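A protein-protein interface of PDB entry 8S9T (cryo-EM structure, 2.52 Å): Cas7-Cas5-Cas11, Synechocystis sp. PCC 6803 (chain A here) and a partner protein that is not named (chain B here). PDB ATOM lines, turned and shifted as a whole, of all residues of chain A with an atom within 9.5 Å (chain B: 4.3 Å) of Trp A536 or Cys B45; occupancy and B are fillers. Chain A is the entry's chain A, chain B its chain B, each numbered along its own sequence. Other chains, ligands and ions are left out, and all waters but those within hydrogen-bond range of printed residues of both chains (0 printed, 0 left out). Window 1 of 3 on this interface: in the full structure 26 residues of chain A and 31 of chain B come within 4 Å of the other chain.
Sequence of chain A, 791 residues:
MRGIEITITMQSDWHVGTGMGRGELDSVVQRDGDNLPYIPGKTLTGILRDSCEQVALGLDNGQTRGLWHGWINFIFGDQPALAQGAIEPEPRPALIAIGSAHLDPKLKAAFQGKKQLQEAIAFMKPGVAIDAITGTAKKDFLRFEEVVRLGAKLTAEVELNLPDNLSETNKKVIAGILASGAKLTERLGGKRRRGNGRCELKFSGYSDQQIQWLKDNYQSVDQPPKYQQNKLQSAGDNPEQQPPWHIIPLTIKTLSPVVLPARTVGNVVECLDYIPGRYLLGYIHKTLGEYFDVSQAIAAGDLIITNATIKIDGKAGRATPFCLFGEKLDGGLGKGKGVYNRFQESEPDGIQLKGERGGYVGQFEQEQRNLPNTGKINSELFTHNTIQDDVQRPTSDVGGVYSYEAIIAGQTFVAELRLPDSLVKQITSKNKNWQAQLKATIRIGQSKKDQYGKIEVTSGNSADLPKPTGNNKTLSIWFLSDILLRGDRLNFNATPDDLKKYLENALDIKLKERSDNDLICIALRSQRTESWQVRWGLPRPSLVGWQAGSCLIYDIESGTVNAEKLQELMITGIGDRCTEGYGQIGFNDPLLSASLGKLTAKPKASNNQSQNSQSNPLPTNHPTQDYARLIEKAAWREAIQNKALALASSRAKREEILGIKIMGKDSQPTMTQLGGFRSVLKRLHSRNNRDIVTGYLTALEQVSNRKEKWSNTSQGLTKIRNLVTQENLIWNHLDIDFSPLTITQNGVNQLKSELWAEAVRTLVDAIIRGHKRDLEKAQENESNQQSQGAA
The backbone NH (N) of Leu A232 is in hydrogen-bond range of the side-chain amide oxygen (OE1) of Gln B43, 2.8 Å away.
O of Gln B43 lies close to O of Arg A535.
NE1 of Trp A536 sits at hydrogen-bond distance from O of Ser B41 (2.5 Å).
NE2 of Gln A533 is in hydrogen-bond range of O of Pro B42 (3.3 Å).
OE1 of Gln A533 sits at hydrogen-bond distance from N of Arg A535, at 3.1 Å.
The backbone carbonyl oxygen of Leu A538 is in hydrogen-bond range of the backbone NH of Gln A533, 3.0 Å away.
N of Phe B71 is in hydrogen-bond range of O of Tyr B40 (2.9 Å).
OE1 of Gln A533 lies within hydrogen-bond range of N of Trp A536 (3.0 Å).
Of chain B, only Tyr B40 (3.4 Å), Ser B41 (2.5 Å), Gln B43 (3.8 Å), Lys B44 (3.5 Å) and Cys B45 (3.5 Å) come within 4 Å of Trp A536.
Of chain A, only Trp A536 comes within 4 Å of Cys B45.
Printed residues of chain B within 4 Å of Leu A232: Gln B43 (2.8 Å).
Printed residues of chain A within 4 Å of Pro B42: Gln A533 and Arg A535.
Printed residues of chain B within 4 Å of Arg A535: Pro B42 (3.5 Å) and Gln B43 (3.0 Å).
Pro A541 touches none of the printed residues of chain B.
Asn A230 touches none of the printed residues of chain B.
The nearest residue of chain B that does not touch Trp A536 is Pro B42 (4.1 Å).
The nearest residue of chain A that does not touch Cys B45 is Leu A538 (4.5 Å).
Of the 19 printed residues of chain A, 4 touch a printed residue of chain B.
Printed residues of chain A that touch a printed residue of chain B: Leu A232, Gln A533, Arg A535 and Trp A536.
Hydrophobic or aromatic side chains of chain A that line the printed part of chain B: Leu A232 and Trp A536.
Printed residues of chain B that touch a printed residue of chain A: Tyr B40, Ser B41, Pro B42, Gln B43, Lys B44 and Cys B45.
Hydrophobic or aromatic side chains of chain B that line the printed part of chain A: Tyr B40.
Among the printed residues, 9 pairs touch across the chains.
Among the printed residues, no Asp or Glu carboxylate lies within 4 Å of a Lys or Arg side-chain nitrogen of the other chain.
Among the printed residues, merely in contact across the chains: Arg A535 with Pro B42 (3.5 Å), Trp A536 with Tyr B40 (3.4 Å), Trp A536 with Gln B43 (3.8 Å), Trp A536 with Lys B44 (3.5 Å) and Trp A536 with Cys B45 (3.5 Å).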
ATOM      1  N   GLU A  90      30.651   2.265   9.940  1.00  0.00           N
ATOM      2  CA  GLU A  90      29.291   2.573  10.355  1.00  0.00           C
ATOM      3  C   GLU A  90      28.446   2.933   9.143  1.00  0.00           C
ATOM      4  O   GLU A  90      28.950   3.540   8.193  1.00  0.00           O
ATOM      5  CB  GLU A  90      29.270   3.728  11.351  1.00  0.00           C
ATOM      6  CG  GLU A  90      29.820   3.387  12.706  1.00  0.00           C
ATOM      7  CD  GLU A  90      29.943   4.596  13.607  1.00  0.00           C
ATOM      8  OE1 GLU A  90      29.044   5.460  13.574  1.00  0.00           O
ATOM      9  OE2 GLU A  90      30.944   4.682  14.350  1.00  0.00           O
ATOM     10  N   GLN A 229      30.289  11.368  12.737  1.00  0.00           N
ATOM     11  CA  GLN A 229      29.275  12.032  13.538  1.00  0.00           C
ATOM     12  C   GLN A 229      29.718  13.431  13.951  1.00  0.00           C
ATOM     13  O   GLN A 229      30.908  13.717  14.101  1.00  0.00           O
ATOM     14  CB  GLN A 229      28.938  11.221  14.786  1.00  0.00           C
ATOM     15  CG  GLN A 229      28.313   9.880  14.521  1.00  0.00           C
ATOM     16  CD  GLN A 229      27.163   9.591  15.470  1.00  0.00           C
ATOM     17  OE1 GLN A 229      26.548  10.510  16.012  1.00  0.00           O
ATOM     18  NE2 GLN A 229      26.856   8.315  15.661  1.00  0.00           N
ATOM     19  N   ASN A 230      28.737  14.311  14.113  1.00  0.00           N
ATOM     20  CA  ASN A 230      28.919  15.535  14.883  1.00  0.00           C
ATOM     21  C   ASN A 230      29.019  15.181  16.360  1.00  0.00           C
ATOM     22  O   ASN A 230      28.048  14.712  16.957  1.00  0.00           O
ATOM     23  CB  ASN A 230      27.756  16.487  14.634  1.00  0.00           C
ATOM     24  CG  ASN A 230      27.737  17.019  13.229  1.00  0.00           C
ATOM     25  OD1 ASN A 230      28.782  17.271  12.637  1.00  0.00           O
ATOM     26  ND2 ASN A 230      26.542  17.199  12.682  1.00  0.00           N
ATOM     27  N   LEU A 232      29.481  15.821  20.474  1.00  0.00           N
ATOM     28  CA  LEU A 232      29.254  16.776  21.548  1.00  0.00           C
ATOM     29  C   LEU A 232      30.532  17.480  21.978  1.00  0.00           C
ATOM     30  O   LEU A 232      31.640  16.956  21.845  1.00  0.00           O
ATOM     31  CB  LEU A 232      28.646  16.071  22.759  1.00  0.00           C
ATOM     32  CG  LEU A 232      27.254  15.480  22.592  1.00  0.00           C
ATOM     33  CD1 LEU A 232      26.858  14.694  23.822  1.00  0.00           C
ATOM     34  CD2 LEU A 232      26.273  16.589  22.304  1.00  0.00           C
ATOM     35  N   ARG A 486      16.371   2.000  39.799  1.00  0.00           N
ATOM     36  CA  ARG A 486      17.338   0.965  40.122  1.00  0.00           C
ATOM     37  C   ARG A 486      16.842   0.139  41.297  1.00  0.00           C
ATOM     38  O   ARG A 486      16.348   0.679  42.287  1.00  0.00           O
ATOM     39  CB  ARG A 486      18.684   1.579  40.490  1.00  0.00           C
ATOM     40  CG  ARG A 486      19.323   2.452  39.454  1.00  0.00           C
ATOM     41  CD  ARG A 486      19.715   1.671  38.255  1.00  0.00           C
ATOM     42  NE  ARG A 486      20.305   2.528  37.244  1.00  0.00           N
ATOM     43  CZ  ARG A 486      21.069   2.087  36.260  1.00  0.00           C
ATOM     44  NH1 ARG A 486      21.355   0.802  36.175  1.00  0.00           N
ATOM     45  NH2 ARG A 486      21.558   2.930  35.378  1.00  0.00           N
ATOM     46  N   SER A 531      14.706   1.314  23.431  1.00  0.00           N
ATOM     47  CA  SER A 531      15.485   2.273  22.628  1.00  0.00           C
ATOM     48  C   SER A 531      16.910   1.983  22.127  1.00  0.00           C
ATOM     49  O   SER A 531      17.578   1.053  22.575  1.00  0.00           O
ATOM     50  CB  SER A 531      15.592   3.574  23.422  1.00  0.00           C
ATOM     51  OG  SER A 531      14.332   4.026  23.849  1.00  0.00           O
ATOM     52  N   TRP A 532      17.344   2.797  21.155  1.00  0.00           N
ATOM     53  CA  TRP A 532      18.699   2.993  20.636  1.00  0.00           C
ATOM     54  C   TRP A 532      19.376   4.189  21.298  1.00  0.00           C
ATOM     55  O   TRP A 532      18.733   5.038  21.906  1.00  0.00           O
ATOM     56  CB  TRP A 532      18.705   3.220  19.123  1.00  0.00           C
ATOM     57  CG  TRP A 532      19.998   2.838  18.388  1.00  0.00           C
ATOM     58  CD1 TRP A 532      20.911   3.708  17.878  1.00  0.00           C
ATOM     59  CD2 TRP A 532      20.479   1.534  18.062  1.00  0.00           C
ATOM     60  NE1 TRP A 532      21.916   3.042  17.265  1.00  0.00           N
ATOM     61  CE2 TRP A 532      21.687   1.701  17.369  1.00  0.00           C
ATOM     62  CE3 TRP A 532      20.006   0.242  18.280  1.00  0.00           C
ATOM     63  CZ2 TRP A 532      22.414   0.637  16.885  1.00  0.00           C
ATOM     64  CZ3 TRP A 532      20.740  -0.810  17.809  1.00  0.00           C
ATOM     65  CH2 TRP A 532      21.929  -0.610  17.124  1.00  0.00           C
ATOM     66  N   GLN A 533      20.687   4.293  21.092  1.00  0.00           N
ATOM     67  CA  GLN A 533      21.474   5.455  21.488  1.00  0.00           C
ATOM     68  C   GLN A 533      22.246   5.750  20.206  1.00  0.00           C
ATOM     69  O   GLN A 533      23.234   5.083  19.904  1.00  0.00           O
ATOM     70  CB  GLN A 533      22.387   5.124  22.670  1.00  0.00           C
ATOM     71  CG  GLN A 533      22.526   6.180  23.779  1.00  0.00           C
ATOM     72  CD  GLN A 533      23.272   7.424  23.404  1.00  0.00           C
ATOM     73  OE1 GLN A 533      23.601   7.651  22.256  1.00  0.00           O
ATOM     74  NE2 GLN A 533      23.523   8.259  24.386  1.00  0.00           N
ATOM     75  N   VAL A 534      21.799   6.774  19.479  1.00  0.00           N
ATOM     76  CA  VAL A 534      22.396   7.194  18.207  1.00  0.00           C
ATOM     77  C   VAL A 534      23.858   7.634  18.323  1.00  0.00           C
ATOM     78  O   VAL A 534      24.675   7.309  17.456  1.00  0.00           O
ATOM     79  CB  VAL A 534      21.532   8.303  17.589  1.00  0.00           C
ATOM     80  CG1 VAL A 534      22.124   8.782  16.303  1.00  0.00           C
ATOM     81  CG2 VAL A 534      20.136   7.821  17.403  1.00  0.00           C
ATOM     82  N   ARG A 535      24.219   8.386  19.358  1.00  0.00           N
ATOM     83  CA  ARG A 535      25.633   8.701  19.549  1.00  0.00           C
ATOM     84  C   ARG A 535      26.462   7.475  19.910  1.00  0.00           C
ATOM     85  O   ARG A 535      27.618   7.368  19.492  1.00  0.00           O
ATOM     86  CB  ARG A 535      25.805   9.781  20.607  1.00  0.00           C
ATOM     87  CG  ARG A 535      24.980  10.999  20.382  1.00  0.00           C
ATOM     88  CD  ARG A 535      25.302  12.039  21.413  1.00  0.00           C
ATOM     89  NE  ARG A 535      24.365  13.146  21.362  1.00  0.00           N
ATOM     90  CZ  ARG A 535      24.483  14.183  20.547  1.00  0.00           C
ATOM     91  NH1 ARG A 535      25.515  14.272  19.729  1.00  0.00           N
ATOM     92  NH2 ARG A 535      23.574  15.138  20.563  1.00  0.00           N
ATOM     93  N   TRP A 536      25.913   6.555  20.698  1.00  0.00           N
ATOM     94  CA  TRP A 536      26.630   5.316  20.960  1.00  0.00           C
ATOM     95  C   TRP A 536      26.841   4.513  19.691  1.00  0.00           C
ATOM     96  O   TRP A 536      27.867   3.846  19.534  1.00  0.00           O
ATOM     97  CB  TRP A 536      25.880   4.457  21.969  1.00  0.00           C
ATOM     98  CG  TRP A 536      25.960   4.897  23.360  1.00  0.00           C
ATOM     99  CD1 TRP A 536      26.468   6.055  23.819  1.00  0.00           C
ATOM    100  CD2 TRP A 536      25.516   4.168  24.503  1.00  0.00           C
ATOM    101  NE1 TRP A 536      26.368   6.107  25.179  1.00  0.00           N
ATOM    102  CE2 TRP A 536      25.781   4.957  25.623  1.00  0.00           C
ATOM    103  CE3 TRP A 536      24.899   2.931  24.682  1.00  0.00           C
ATOM    104  CZ2 TRP A 536      25.467   4.556  26.897  1.00  0.00           C
ATOM    105  CZ3 TRP A 536      24.595   2.537  25.952  1.00  0.00           C
ATOM    106  CH2 TRP A 536      24.879   3.341  27.043  1.00  0.00           C
ATOM    107  N   GLY A 537      25.877   4.539  18.784  1.00  0.00           N
ATOM    108  CA  GLY A 537      25.975   3.679  17.644  1.00  0.00           C
ATOM    109  C   GLY A 537      25.466   2.303  17.960  1.00  0.00           C
ATOM    110  O   GLY A 537      25.563   1.400  17.125  1.00  0.00           O
ATOM    111  N   LEU A 538      24.886   2.145  19.138  1.00  0.00           N
ATOM    112  CA  LEU A 538      24.553   0.856  19.713  1.00  0.00           C
ATOM    113  C   LEU A 538      23.261   1.018  20.483  1.00  0.00           C
ATOM    114  O   LEU A 538      22.801   2.139  20.709  1.00  0.00           O
ATOM    115  CB  LEU A 538      25.669   0.392  20.646  1.00  0.00           C
ATOM    116  CG  LEU A 538      26.898  -0.210  20.000  1.00  0.00           C
ATOM    117  CD1 LEU A 538      27.824  -0.668  21.080  1.00  0.00           C
ATOM    118  CD2 LEU A 538      26.481  -1.344  19.106  1.00  0.00           C
ATOM    119  N   PRO A 539      22.629  -0.083  20.865  1.00  0.00           N
ATOM    120  CA  PRO A 539      21.349   0.011  21.563  1.00  0.00           C
ATOM    121  C   PRO A 539      21.519   0.611  22.934  1.00  0.00           C
ATOM    122  O   PRO A 539      22.587   0.534  23.539  1.00  0.00           O
ATOM    123  CB  PRO A 539      20.889  -1.445  21.676  1.00  0.00           C
ATOM    124  CG  PRO A 539      21.668  -2.183  20.758  1.00  0.00           C
ATOM    125  CD  PRO A 539      22.898  -1.453  20.413  1.00  0.00           C
ATOM    126  N   ARG A 540      20.474   1.243  23.412  1.00  0.00           N
ATOM    127  CA  ARG A 540      20.525   1.671  24.788  1.00  0.00           C
ATOM    128  C   ARG A 540      20.273   0.466  25.676  1.00  0.00           C
ATOM    129  O   ARG A 540      19.699  -0.527  25.236  1.00  0.00           O
ATOM    130  CB  ARG A 540      19.429   2.680  25.057  1.00  0.00           C
ATOM    131  CG  ARG A 540      19.779   4.105  25.258  1.00  0.00           C
ATOM    132  CD  ARG A 540      18.475   4.823  25.092  1.00  0.00           C
ATOM    133  NE  ARG A 540      18.282   5.899  26.039  1.00  0.00           N
ATOM    134  CZ  ARG A 540      17.098   6.306  26.468  1.00  0.00           C
ATOM    135  NH1 ARG A 540      15.993   5.704  26.074  1.00  0.00           N
ATOM    136  NH2 ARG A 540      17.034   7.299  27.321  1.00  0.00           N
ATOM    137  N   PRO A 541      20.731   0.500  26.918  1.00  0.00           N
ATOM    138  CA  PRO A 541      20.397  -0.580  27.837  1.00  0.00           C
ATOM    139  C   PRO A 541      18.898  -0.598  28.066  1.00  0.00           C
ATOM    140  O   PRO A 541      18.237   0.438  28.045  1.00  0.00           O
ATOM    141  CB  PRO A 541      21.165  -0.209  29.104  1.00  0.00           C
ATOM    142  CG  PRO A 541      21.415   1.226  28.954  1.00  0.00           C
ATOM    143  CD  PRO A 541      21.710   1.400  27.530  1.00  0.00           C
ATOM    144  N   SER A 542      18.353  -1.778  28.287  1.00  0.00           N
ATOM    145  CA  SER A 542      16.915  -1.872  28.457  1.00  0.00           C
ATOM    146  C   SER A 542      16.526  -1.248  29.790  1.00  0.00           C
ATOM    147  O   SER A 542      17.111  -1.570  30.824  1.00  0.00           O
ATOM    148  CB  SER A 542      16.477  -3.326  28.390  1.00  0.00           C
ATOM    149  OG  SER A 542      15.210  -3.418  27.792  1.00  0.00           O
ATOM    150  N   LEU A 543      15.527  -0.373  29.771  1.00  0.00           N
ATOM    151  CA  LEU A 543      15.103   0.372  30.951  1.00  0.00           C
ATOM    152  C   LEU A 543      13.752  -0.143  31.408  1.00  0.00           C
ATOM    153  O   LEU A 543      12.764  -0.053  30.677  1.00  0.00           O
ATOM    154  CB  LEU A 543      15.035   1.871  30.676  1.00  0.00           C
ATOM    155  CG  LEU A 543      16.241   2.461  29.961  1.00  0.00           C
ATOM    156  CD1 LEU A 543      15.898   3.775  29.307  1.00  0.00           C
ATOM    157  CD2 LEU A 543      17.375   2.603  30.930  1.00  0.00           C
ATOM    158  N   ARG A 577      17.147   8.879  34.730  1.00  0.00           N
ATOM    159  CA  ARG A 577      16.937   9.552  33.440  1.00  0.00           C
ATOM    160  C   ARG A 577      15.757  10.517  33.430  1.00  0.00           C
ATOM    161  O   ARG A 577      15.029  10.637  32.444  1.00  0.00           O
ATOM    162  CB  ARG A 577      16.851   8.547  32.300  1.00  0.00           C
ATOM    163  CG  ARG A 577      18.172   7.888  32.070  1.00  0.00           C
ATOM    164  CD  ARG A 577      18.150   6.914  30.944  1.00  0.00           C
ATOM    165  NE  ARG A 577      18.939   5.751  31.299  1.00  0.00           N
ATOM    166  CZ  ARG A 577      20.042   5.383  30.673  1.00  0.00           C
ATOM    167  NH1 ARG A 577      20.413   6.000  29.571  1.00  0.00           N
ATOM    168  NH2 ARG A 577      20.701   4.319  31.083  1.00  0.00           N
ATOM    169  N   LEU B  38      32.245  -2.346  30.689  1.00  0.00           N
ATOM    170  CA  LEU B  38      31.390  -1.645  29.749  1.00  0.00           C
ATOM    171  C   LEU B  38      31.038  -0.296  30.355  1.00  0.00           C
ATOM    172  O   LEU B  38      30.375  -0.234  31.390  1.00  0.00           O
ATOM    173  CB  LEU B  38      30.153  -2.489  29.442  1.00  0.00           C
ATOM    174  CG  LEU B  38      29.244  -2.046  28.312  1.00  0.00           C
ATOM    175  CD1 LEU B  38      30.051  -2.133  27.073  1.00  0.00           C
ATOM    176  CD2 LEU B  38      28.082  -2.989  28.199  1.00  0.00           C
ATOM    177  N   LEU B  39      31.487   0.777  29.720  1.00  0.00           N
ATOM    178  CA  LEU B  39      31.383   2.123  30.261  1.00  0.00           C
ATOM    179  C   LEU B  39      30.344   2.893  29.465  1.00  0.00           C
ATOM    180  O   LEU B  39      30.337   2.852  28.234  1.00  0.00           O
ATOM    181  CB  LEU B  39      32.721   2.855  30.202  1.00  0.00           C
ATOM    182  CG  LEU B  39      33.957   2.165  30.756  1.00  0.00           C
ATOM    183  CD1 LEU B  39      35.149   3.088  30.631  1.00  0.00           C
ATOM    184  CD2 LEU B  39      33.750   1.742  32.185  1.00  0.00           C
ATOM    185  N   TYR B  40      29.481   3.608  30.174  1.00  0.00           N
ATOM    186  CA  TYR B  40      28.401   4.373  29.574  1.00  0.00           C
ATOM    187  C   TYR B  40      28.621   5.871  29.696  1.00  0.00           C
ATOM    188  O   TYR B  40      28.680   6.404  30.799  1.00  0.00           O
ATOM    189  CB  TYR B  40      27.071   4.002  30.223  1.00  0.00           C
ATOM    190  CG  TYR B  40      26.636   2.571  30.029  1.00  0.00           C
ATOM    191  CD1 TYR B  40      27.178   1.776  29.028  1.00  0.00           C
ATOM    192  CD2 TYR B  40      25.673   2.017  30.844  1.00  0.00           C
ATOM    193  CE1 TYR B  40      26.781   0.474  28.864  1.00  0.00           C
ATOM    194  CE2 TYR B  40      25.269   0.722  30.685  1.00  0.00           C
ATOM    195  CZ  TYR B  40      25.821  -0.045  29.698  1.00  0.00           C
ATOM    196  OH  TYR B  40      25.396  -1.336  29.553  1.00  0.00           O
ATOM    197  N   SER B  41      28.726   6.544  28.562  1.00  0.00           N
ATOM    198  CA  SER B  41      28.960   7.975  28.485  1.00  0.00           C
ATOM    199  C   SER B  41      27.965   8.517  27.474  1.00  0.00           C
ATOM    200  O   SER B  41      27.379   7.753  26.702  1.00  0.00           O
ATOM    201  CB  SER B  41      30.393   8.327  28.050  1.00  0.00           C
ATOM    202  OG  SER B  41      31.330   7.354  28.449  1.00  0.00           O
ATOM    203  N   PRO B  42      27.739   9.829  27.461  1.00  0.00           N
ATOM    204  CA  PRO B  42      26.758  10.386  26.523  1.00  0.00           C
ATOM    205  C   PRO B  42      27.105  10.157  25.075  1.00  0.00           C
ATOM    206  O   PRO B  42      26.208  10.116  24.225  1.00  0.00           O
ATOM    207  CB  PRO B  42      26.749  11.881  26.866  1.00  0.00           C
ATOM    208  CG  PRO B  42      27.709  12.067  27.946  1.00  0.00           C
ATOM    209  CD  PRO B  42      28.027  10.773  28.550  1.00  0.00           C
ATOM    210  N   GLN B  43      28.389  10.027  24.764  1.00  0.00           N
ATOM    211  CA  GLN B  43      28.835   9.884  23.396  1.00  0.00           C
ATOM    212  C   GLN B  43      29.311   8.490  23.040  1.00  0.00           C
ATOM    213  O   GLN B  43      29.351   8.158  21.855  1.00  0.00           O
ATOM    214  CB  GLN B  43      30.001  10.855  23.164  1.00  0.00           C
ATOM    215  CG  GLN B  43      29.602  12.290  22.933  1.00  0.00           C
ATOM    216  CD  GLN B  43      29.666  12.701  21.484  1.00  0.00           C
ATOM    217  OE1 GLN B  43      30.609  13.365  21.083  1.00  0.00           O
ATOM    218  NE2 GLN B  43      28.674  12.310  20.690  1.00  0.00           N
ATOM    219  N   LYS B  44      29.660   7.668  24.019  1.00  0.00           N
ATOM    220  CA  LYS B  44      30.268   6.388  23.707  1.00  0.00           C
ATOM    221  C   LYS B  44      29.901   5.294  24.690  1.00  0.00           C
ATOM    222  O   LYS B  44      29.764   5.533  25.886  1.00  0.00           O
ATOM    223  CB  LYS B  44      31.803   6.480  23.644  1.00  0.00           C
ATOM    224  CG  LYS B  44      32.382   7.820  23.997  1.00  0.00           C
ATOM    225  CD  LYS B  44      33.882   7.763  24.088  1.00  0.00           C
ATOM    226  CE  LYS B  44      34.419   9.002  24.757  1.00  0.00           C
ATOM    227  NZ  LYS B  44      35.902   9.057  24.708  1.00  0.00           N
ATOM    228  N   CYS B  45      29.735   4.098  24.159  1.00  0.00           N
ATOM    229  CA  CYS B  45      29.580   2.888  24.946  1.00  0.00           C
ATOM    230  C   CYS B  45      30.829   2.150  24.501  1.00  0.00           C
ATOM    231  O   CYS B  45      30.938   1.751  23.340  1.00  0.00           O
ATOM    232  CB  CYS B  45      28.305   2.118  24.618  1.00  0.00           C
ATOM    233  SG  CYS B  45      28.129   0.581  25.526  1.00  0.00           S
ATOM    234  N   GLU B  46      31.773   1.988  25.404  1.00  0.00           N
ATOM    235  CA  GLU B  46      33.018   1.322  25.076  1.00  0.00           C
ATOM    236  C   GLU B  46      33.327   0.162  26.003  1.00  0.00           C
ATOM    237  O   GLU B  46      33.108   0.238  27.212  1.00  0.00           O
ATOM    238  CB  GLU B  46      34.150   2.338  25.065  1.00  0.00           C
ATOM    239  CG  GLU B  46      34.416   3.003  26.362  1.00  0.00           C
ATOM    240  CD  GLU B  46      35.453   4.079  26.216  1.00  0.00           C
ATOM    241  OE1 GLU B  46      35.200   5.211  26.677  1.00  0.00           O
ATOM    242  OE2 GLU B  46      36.515   3.798  25.623  1.00  0.00           O
ATOM    243  N   PHE B  71      28.963   7.927  33.258  1.00  0.00           N
ATOM    244  CA  PHE B  71      27.870   7.973  34.216  1.00  0.00           C
ATOM    245  C   PHE B  71      27.449   6.601  34.721  1.00  0.00           C
ATOM    246  O   PHE B  71      26.754   6.525  35.736  1.00  0.00           O
ATOM    247  CB  PHE B  71      26.665   8.735  33.629  1.00  0.00           C
ATOM    248  CG  PHE B  71      26.043   8.109  32.411  1.00  0.00           C
ATOM    249  CD1 PHE B  71      25.224   7.004  32.500  1.00  0.00           C
ATOM    250  CD2 PHE B  71      26.251   8.664  31.172  1.00  0.00           C
ATOM    251  CE1 PHE B  71      24.652   6.456  31.375  1.00  0.00           C
ATOM    252  CE2 PHE B  71      25.678   8.123  30.058  1.00  0.00           C
ATOM    253  CZ  PHE B  71      24.875   7.017  30.163  1.00  0.00           C
